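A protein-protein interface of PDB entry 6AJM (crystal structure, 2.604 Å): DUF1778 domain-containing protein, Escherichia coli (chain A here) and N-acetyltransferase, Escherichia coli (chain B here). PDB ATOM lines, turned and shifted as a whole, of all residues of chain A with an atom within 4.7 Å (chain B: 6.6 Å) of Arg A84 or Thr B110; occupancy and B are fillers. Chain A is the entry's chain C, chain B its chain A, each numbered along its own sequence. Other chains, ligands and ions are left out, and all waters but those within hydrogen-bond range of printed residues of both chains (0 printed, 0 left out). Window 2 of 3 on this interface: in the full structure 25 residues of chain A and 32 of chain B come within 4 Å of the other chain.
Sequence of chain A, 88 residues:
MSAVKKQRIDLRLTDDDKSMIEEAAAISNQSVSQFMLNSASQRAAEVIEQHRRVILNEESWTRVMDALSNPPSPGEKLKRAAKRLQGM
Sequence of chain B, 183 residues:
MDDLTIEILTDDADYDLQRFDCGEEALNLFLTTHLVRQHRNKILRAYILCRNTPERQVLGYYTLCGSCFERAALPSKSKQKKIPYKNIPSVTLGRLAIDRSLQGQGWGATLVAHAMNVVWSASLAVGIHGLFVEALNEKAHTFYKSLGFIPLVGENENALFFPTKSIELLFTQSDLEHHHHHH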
ATOM      1  N   ARG A  80     -24.696 -28.119 -16.384  1.00  0.00           N
ATOM      2  CA  ARG A  80     -23.561 -27.502 -17.066  1.00  0.00           C
ATOM      3  C   ARG A  80     -23.153 -26.205 -16.384  1.00  0.00           C
ATOM      4  O   ARG A  80     -21.972 -25.842 -16.397  1.00  0.00           O
ATOM      5  CB  ARG A  80     -23.911 -27.260 -18.542  1.00  0.00           C
ATOM      6  CG  ARG A  80     -22.821 -27.691 -19.546  1.00  0.00           C
ATOM      7  CD  ARG A  80     -23.359 -28.591 -20.681  1.00  0.00           C
ATOM      8  NE  ARG A  80     -23.798 -29.914 -20.213  1.00  0.00           N
ATOM      9  CZ  ARG A  80     -23.201 -31.072 -20.506  1.00  0.00           C
ATOM     10  NH1 ARG A  80     -22.120 -31.100 -21.280  1.00  0.00           N
ATOM     11  NH2 ARG A  80     -23.691 -32.212 -20.021  1.00  0.00           N
ATOM     12  N   ALA A  81     -24.111 -25.496 -15.783  1.00  0.00           N
ATOM     13  CA  ALA A  81     -23.758 -24.297 -15.014  1.00  0.00           C
ATOM     14  C   ALA A  81     -23.192 -24.651 -13.639  1.00  0.00           C
ATOM     15  O   ALA A  81     -22.256 -23.994 -13.139  1.00  0.00           O
ATOM     16  CB  ALA A  81     -24.971 -23.379 -14.850  1.00  0.00           C
ATOM     17  N   ALA A  82     -23.772 -25.678 -13.013  1.00  0.00           N
ATOM     18  CA  ALA A  82     -23.267 -26.160 -11.737  1.00  0.00           C
ATOM     19  C   ALA A  82     -21.796 -26.535 -11.834  1.00  0.00           C
ATOM     20  O   ALA A  82     -21.011 -26.236 -10.929  1.00  0.00           O
ATOM     21  CB  ALA A  82     -24.091 -27.358 -11.264  1.00  0.00           C
ATOM     22  N   LYS A  83     -21.401 -27.204 -12.920  1.00  0.00           N
ATOM     23  CA  LYS A  83     -19.988 -27.541 -13.071  1.00  0.00           C
ATOM     24  C   LYS A  83     -19.138 -26.332 -13.447  1.00  0.00           C
ATOM     25  O   LYS A  83     -17.917 -26.380 -13.280  1.00  0.00           O
ATOM     26  CB  LYS A  83     -19.791 -28.669 -14.094  1.00  0.00           C
ATOM     27  CG  LYS A  83     -18.584 -29.559 -13.760  1.00  0.00           C
ATOM     28  CD  LYS A  83     -18.654 -30.932 -14.427  1.00  0.00           C
ATOM     29  CE  LYS A  83     -17.375 -31.730 -14.179  1.00  0.00           C
ATOM     30  NZ  LYS A  83     -17.349 -33.071 -14.847  1.00  0.00           N
ATOM     31  N   ARG A  84     -19.739 -25.235 -13.916  1.00  0.00           N
ATOM     32  CA  ARG A  84     -18.958 -24.011 -14.075  1.00  0.00           C
ATOM     33  C   ARG A  84     -18.550 -23.448 -12.717  1.00  0.00           C
ATOM     34  O   ARG A  84     -17.361 -23.222 -12.467  1.00  0.00           O
ATOM     35  CB  ARG A  84     -19.719 -22.963 -14.896  1.00  0.00           C
ATOM     36  CG  ARG A  84     -19.512 -23.094 -16.414  1.00  0.00           C
ATOM     37  CD  ARG A  84     -20.096 -21.919 -17.201  1.00  0.00           C
ATOM     38  NE  ARG A  84     -21.560 -21.945 -17.311  1.00  0.00           N
ATOM     39  CZ  ARG A  84     -22.236 -22.587 -18.264  1.00  0.00           C
ATOM     40  NH1 ARG A  84     -21.584 -23.281 -19.193  1.00  0.00           N
ATOM     41  NH2 ARG A  84     -23.566 -22.540 -18.287  1.00  0.00           N
ATOM     42  N   LEU A  85     -19.509 -23.251 -11.803  1.00  0.00           N
ATOM     43  CA  LEU A  85     -19.059 -22.580 -10.575  1.00  0.00           C
ATOM     44  C   LEU A  85     -18.211 -23.467  -9.662  1.00  0.00           C
ATOM     45  O   LEU A  85     -17.602 -22.955  -8.717  1.00  0.00           O
ATOM     46  CB  LEU A  85     -20.230 -21.999  -9.775  1.00  0.00           C
ATOM     47  CG  LEU A  85     -21.104 -22.854  -8.883  1.00  0.00           C
ATOM     48  CD1 LEU A  85     -21.747 -21.943  -7.892  1.00  0.00           C
ATOM     49  CD2 LEU A  85     -22.149 -23.545  -9.704  1.00  0.00           C
ATOM     50  N   GLN A  86     -18.119 -24.762  -9.925  1.00  0.00           N
ATOM     51  CA  GLN A  86     -17.191 -25.589  -9.163  1.00  0.00           C
ATOM     52  C   GLN A  86     -15.756 -25.284  -9.584  1.00  0.00           C
ATOM     53  O   GLN A  86     -14.949 -24.832  -8.772  1.00  0.00           O
ATOM     54  CB  GLN A  86     -17.507 -27.073  -9.347  1.00  0.00           C
ATOM     55  CG  GLN A  86     -18.814 -27.507  -8.679  1.00  0.00           C
ATOM     56  CD  GLN A  86     -19.046 -29.008  -8.752  1.00  0.00           C
ATOM     57  OE1 GLN A  86     -18.343 -29.719  -9.479  1.00  0.00           O
ATOM     58  NE2 GLN A  86     -20.034 -29.500  -7.996  1.00  0.00           N
ATOM     59  N   ILE B   6     -18.388 -14.468  -6.526  1.00  0.00           N
ATOM     60  CA  ILE B   6     -19.737 -14.289  -6.024  1.00  0.00           C
ATOM     61  C   ILE B   6     -19.610 -14.240  -4.513  1.00  0.00           C
ATOM     62  O   ILE B   6     -19.252 -15.234  -3.877  1.00  0.00           O
ATOM     63  CB  ILE B   6     -20.678 -15.410  -6.473  1.00  0.00           C
ATOM     64  CG1 ILE B   6     -20.593 -15.584  -7.989  1.00  0.00           C
ATOM     65  CG2 ILE B   6     -22.098 -15.106  -6.039  1.00  0.00           C
ATOM     66  CD1 ILE B   6     -21.704 -16.393  -8.574  1.00  0.00           C
ATOM     67  N   LEU B  49     -21.979 -10.541  -7.877  1.00  0.00           N
ATOM     68  CA  LEU B  49     -21.014 -11.031  -8.850  1.00  0.00           C
ATOM     69  C   LEU B  49     -20.151  -9.849  -9.252  1.00  0.00           C
ATOM     70  O   LEU B  49     -20.633  -8.929  -9.922  1.00  0.00           O
ATOM     71  CB  LEU B  49     -21.730 -11.624 -10.054  1.00  0.00           C
ATOM     72  CG  LEU B  49     -20.839 -11.785 -11.257  1.00  0.00           C
ATOM     73  CD1 LEU B  49     -19.751 -12.796 -10.899  1.00  0.00           C
ATOM     74  CD2 LEU B  49     -21.671 -12.184 -12.462  1.00  0.00           C
ATOM     75  N   TYR B  62     -27.872 -11.338  -7.287  1.00  0.00           N
ATOM     76  CA  TYR B  62     -29.131 -12.018  -7.028  1.00  0.00           C
ATOM     77  C   TYR B  62     -29.504 -11.836  -5.566  1.00  0.00           C
ATOM     78  O   TYR B  62     -28.683 -11.435  -4.738  1.00  0.00           O
ATOM     79  CB  TYR B  62     -29.085 -13.502  -7.435  1.00  0.00           C
ATOM     80  CG  TYR B  62     -28.282 -14.434  -6.574  1.00  0.00           C
ATOM     81  CD1 TYR B  62     -28.827 -14.977  -5.420  1.00  0.00           C
ATOM     82  CD2 TYR B  62     -26.996 -14.829  -6.948  1.00  0.00           C
ATOM     83  CE1 TYR B  62     -28.095 -15.858  -4.632  1.00  0.00           C
ATOM     84  CE2 TYR B  62     -26.255 -15.720  -6.162  1.00  0.00           C
ATOM     85  CZ  TYR B  62     -26.812 -16.228  -5.020  1.00  0.00           C
ATOM     86  OH  TYR B  62     -26.079 -17.093  -4.252  1.00  0.00           O
ATOM     87  N   GLN B 105     -23.550 -15.343 -22.002  1.00  0.00           N
ATOM     88  CA  GLN B 105     -22.351 -16.007 -21.503  1.00  0.00           C
ATOM     89  C   GLN B 105     -22.659 -16.968 -20.361  1.00  0.00           C
ATOM     90  O   GLN B 105     -21.756 -17.303 -19.594  1.00  0.00           O
ATOM     91  CB  GLN B 105     -21.302 -14.974 -21.056  1.00  0.00           C
ATOM     92  CG  GLN B 105     -20.507 -14.341 -22.209  1.00  0.00           C
ATOM     93  CD  GLN B 105     -19.595 -13.197 -21.773  1.00  0.00           C
ATOM     94  OE1 GLN B 105     -19.820 -12.037 -22.138  1.00  0.00           O
ATOM     95  NE2 GLN B 105     -18.550 -13.524 -21.000  1.00  0.00           N
ATOM     96  N   GLY B 106     -23.913 -17.402 -20.216  1.00  0.00           N
ATOM     97  CA  GLY B 106     -24.265 -18.364 -19.198  1.00  0.00           C
ATOM     98  C   GLY B 106     -24.099 -17.894 -17.774  1.00  0.00           C
ATOM     99  O   GLY B 106     -24.352 -18.678 -16.854  1.00  0.00           O
ATOM    100  N   TRP B 107     -23.696 -16.641 -17.553  1.00  0.00           N
ATOM    101  CA  TRP B 107     -23.557 -16.156 -16.188  1.00  0.00           C
ATOM    102  C   TRP B 107     -24.882 -16.146 -15.442  1.00  0.00           C
ATOM    103  O   TRP B 107     -24.902 -16.360 -14.224  1.00  0.00           O
ATOM    104  CB  TRP B 107     -22.940 -14.774 -16.189  1.00  0.00           C
ATOM    105  CG  TRP B 107     -21.473 -14.863 -16.361  1.00  0.00           C
ATOM    106  CD1 TRP B 107     -20.748 -14.525 -17.471  1.00  0.00           C
ATOM    107  CD2 TRP B 107     -20.535 -15.352 -15.403  1.00  0.00           C
ATOM    108  NE1 TRP B 107     -19.417 -14.754 -17.249  1.00  0.00           N
ATOM    109  CE2 TRP B 107     -19.255 -15.260 -15.987  1.00  0.00           C
ATOM    110  CE3 TRP B 107     -20.652 -15.832 -14.095  1.00  0.00           C
ATOM    111  CZ2 TRP B 107     -18.101 -15.650 -15.314  1.00  0.00           C
ATOM    112  CZ3 TRP B 107     -19.519 -16.207 -13.426  1.00  0.00           C
ATOM    113  CH2 TRP B 107     -18.256 -16.126 -14.039  1.00  0.00           C
ATOM    114  N   GLY B 108     -25.996 -15.922 -16.134  1.00  0.00           N
ATOM    115  CA  GLY B 108     -27.282 -16.106 -15.479  1.00  0.00           C
ATOM    116  C   GLY B 108     -27.423 -17.488 -14.862  1.00  0.00           C
ATOM    117  O   GLY B 108     -27.752 -17.628 -13.683  1.00  0.00           O
ATOM    118  N   ALA B 109     -27.113 -18.522 -15.645  1.00  0.00           N
ATOM    119  CA  ALA B 109     -27.215 -19.893 -15.171  1.00  0.00           C
ATOM    120  C   ALA B 109     -26.257 -20.171 -14.012  1.00  0.00           C
ATOM    121  O   ALA B 109     -26.640 -20.819 -13.034  1.00  0.00           O
ATOM    122  CB  ALA B 109     -26.966 -20.873 -16.321  1.00  0.00           C
ATOM    123  N   THR B 110     -25.005 -19.702 -14.092  1.00  0.00           N
ATOM    124  CA  THR B 110     -24.083 -20.007 -12.999  1.00  0.00           C
ATOM    125  C   THR B 110     -24.497 -19.280 -11.717  1.00  0.00           C
ATOM    126  O   THR B 110     -24.380 -19.841 -10.622  1.00  0.00           O
ATOM    127  CB  THR B 110     -22.624 -19.699 -13.389  1.00  0.00           C
ATOM    128  OG1 THR B 110     -22.347 -18.307 -13.276  1.00  0.00           O
ATOM    129  CG2 THR B 110     -22.333 -20.143 -14.816  1.00  0.00           C
ATOM    130  N   LEU B 111     -25.034 -18.062 -11.824  1.00  0.00           N
ATOM    131  CA  LEU B 111     -25.593 -17.423 -10.636  1.00  0.00           C
ATOM    132  C   LEU B 111     -26.740 -18.241 -10.063  1.00  0.00           C
ATOM    133  O   LEU B 111     -26.825 -18.440  -8.846  1.00  0.00           O
ATOM    134  CB  LEU B 111     -26.066 -16.006 -10.956  1.00  0.00           C
ATOM    135  CG  LEU B 111     -25.149 -14.916 -10.426  1.00  0.00           C
ATOM    136  CD1 LEU B 111     -23.806 -15.022 -11.110  1.00  0.00           C
ATOM    137  CD2 LEU B 111     -25.785 -13.565 -10.662  1.00  0.00           C
ATOM    138  N   VAL B 112     -27.643 -18.714 -10.925  1.00  0.00           N
ATOM    139  CA  VAL B 112     -28.735 -19.545 -10.433  1.00  0.00           C
ATOM    140  C   VAL B 112     -28.179 -20.761  -9.705  1.00  0.00           C
ATOM    141  O   VAL B 112     -28.650 -21.125  -8.622  1.00  0.00           O
ATOM    142  CB  VAL B 112     -29.674 -19.947 -11.588  1.00  0.00           C
ATOM    143  CG1 VAL B 112     -30.732 -20.916 -11.098  1.00  0.00           C
ATOM    144  CG2 VAL B 112     -30.324 -18.712 -12.210  1.00  0.00           C
ATOM    145  N   ALA B 113     -27.163 -21.397 -10.277  1.00  0.00           N
ATOM    146  CA  ALA B 113     -26.581 -22.573  -9.641  1.00  0.00           C
ATOM    147  C   ALA B 113     -25.982 -22.213  -8.292  1.00  0.00           C
ATOM    148  O   ALA B 113     -26.073 -22.986  -7.332  1.00  0.00           O
ATOM    149  CB  ALA B 113     -25.511 -23.195 -10.533  1.00  0.00           C
ATOM    150  N   HIS B 114     -25.371 -21.032  -8.203  1.00  0.00           N
ATOM    151  CA  HIS B 114     -24.772 -20.599  -6.949  1.00  0.00           C
ATOM    152  C   HIS B 114     -25.827 -20.378  -5.875  1.00  0.00           C
ATOM    153  O   HIS B 114     -25.649 -20.783  -4.718  1.00  0.00           O
ATOM    154  CB  HIS B 114     -23.994 -19.324  -7.189  1.00  0.00           C
ATOM    155  CG  HIS B 114     -23.318 -18.805  -5.973  1.00  0.00           C
ATOM    156  ND1 HIS B 114     -23.976 -18.060  -5.022  1.00  0.00           N
ATOM    157  CD2 HIS B 114     -22.035 -18.902  -5.557  1.00  0.00           C
ATOM    158  CE1 HIS B 114     -23.130 -17.723  -4.065  1.00  0.00           C
ATOM    159  NE2 HIS B 114     -21.943 -18.214  -4.370  1.00  0.00           N
ATOM    160  N   ALA B 115     -26.909 -19.694  -6.234  1.00  0.00           N
ATOM    161  CA  ALA B 115     -28.032 -19.566  -5.317  1.00  0.00           C
ATOM    162  C   ALA B 115     -28.524 -20.934  -4.868  1.00  0.00           C
ATOM    163  O   ALA B 115     -28.838 -21.129  -3.689  1.00  0.00           O
ATOM    164  CB  ALA B 115     -29.165 -18.782  -5.965  1.00  0.00           C
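Printed residues of chain B within 4 Å of Ala A81: Ala B109 and Thr B110. Printed residues of chain B within 4 Å of Ala A82: Ala B113 (3.9 Å). Printed residues of chain B within 4 Å of Leu A85: Ala B113 and His B114. Trp B107 touches none of the printed residues of chain A. Thr B110 touches just these residues of chain A: Ala A81 (3.8 Å) and Arg A84 (3.2 Å). Of the printed residues of chain A, His B114 touches Leu A85 (3.4 Å). The nearest printed residue of chain A that does not touch Ala B109 is Arg A84 (4.3 Å).
Ala B109 touches Ala A81. Ala A81 touches Thr B110 (CB to N, 3.8 Å). CA of Ala A82 touches CB of Ala B113, at 3.9 Å. NE of Arg A84 touches CG2 of Thr B110, 3.2 Å away. Ala B113 touches Leu A85. CD1 of Leu A85 touches CA of His B114, 3.4 Å away.
The side-chain hydroxyl of Tyr B62 lies within hydrogen-bond range of a ring nitrogen (ND1) of His B114 (2.4 Å). The backbone carbonyl oxygen of Trp B107 lies close to the side-chain hydroxyl of Thr B110, 3.3 Å away.
Printed residues of chain A that touch a printed residue of chain B: Ala A81, Ala A82, Arg A84 and Leu A85. Hydrophobic or aromatic side chains of chain B that line the printed part of chain A: Ala B109, Ala B113 and His B114. Among the printed residues, 6 pairs touch across the chains.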
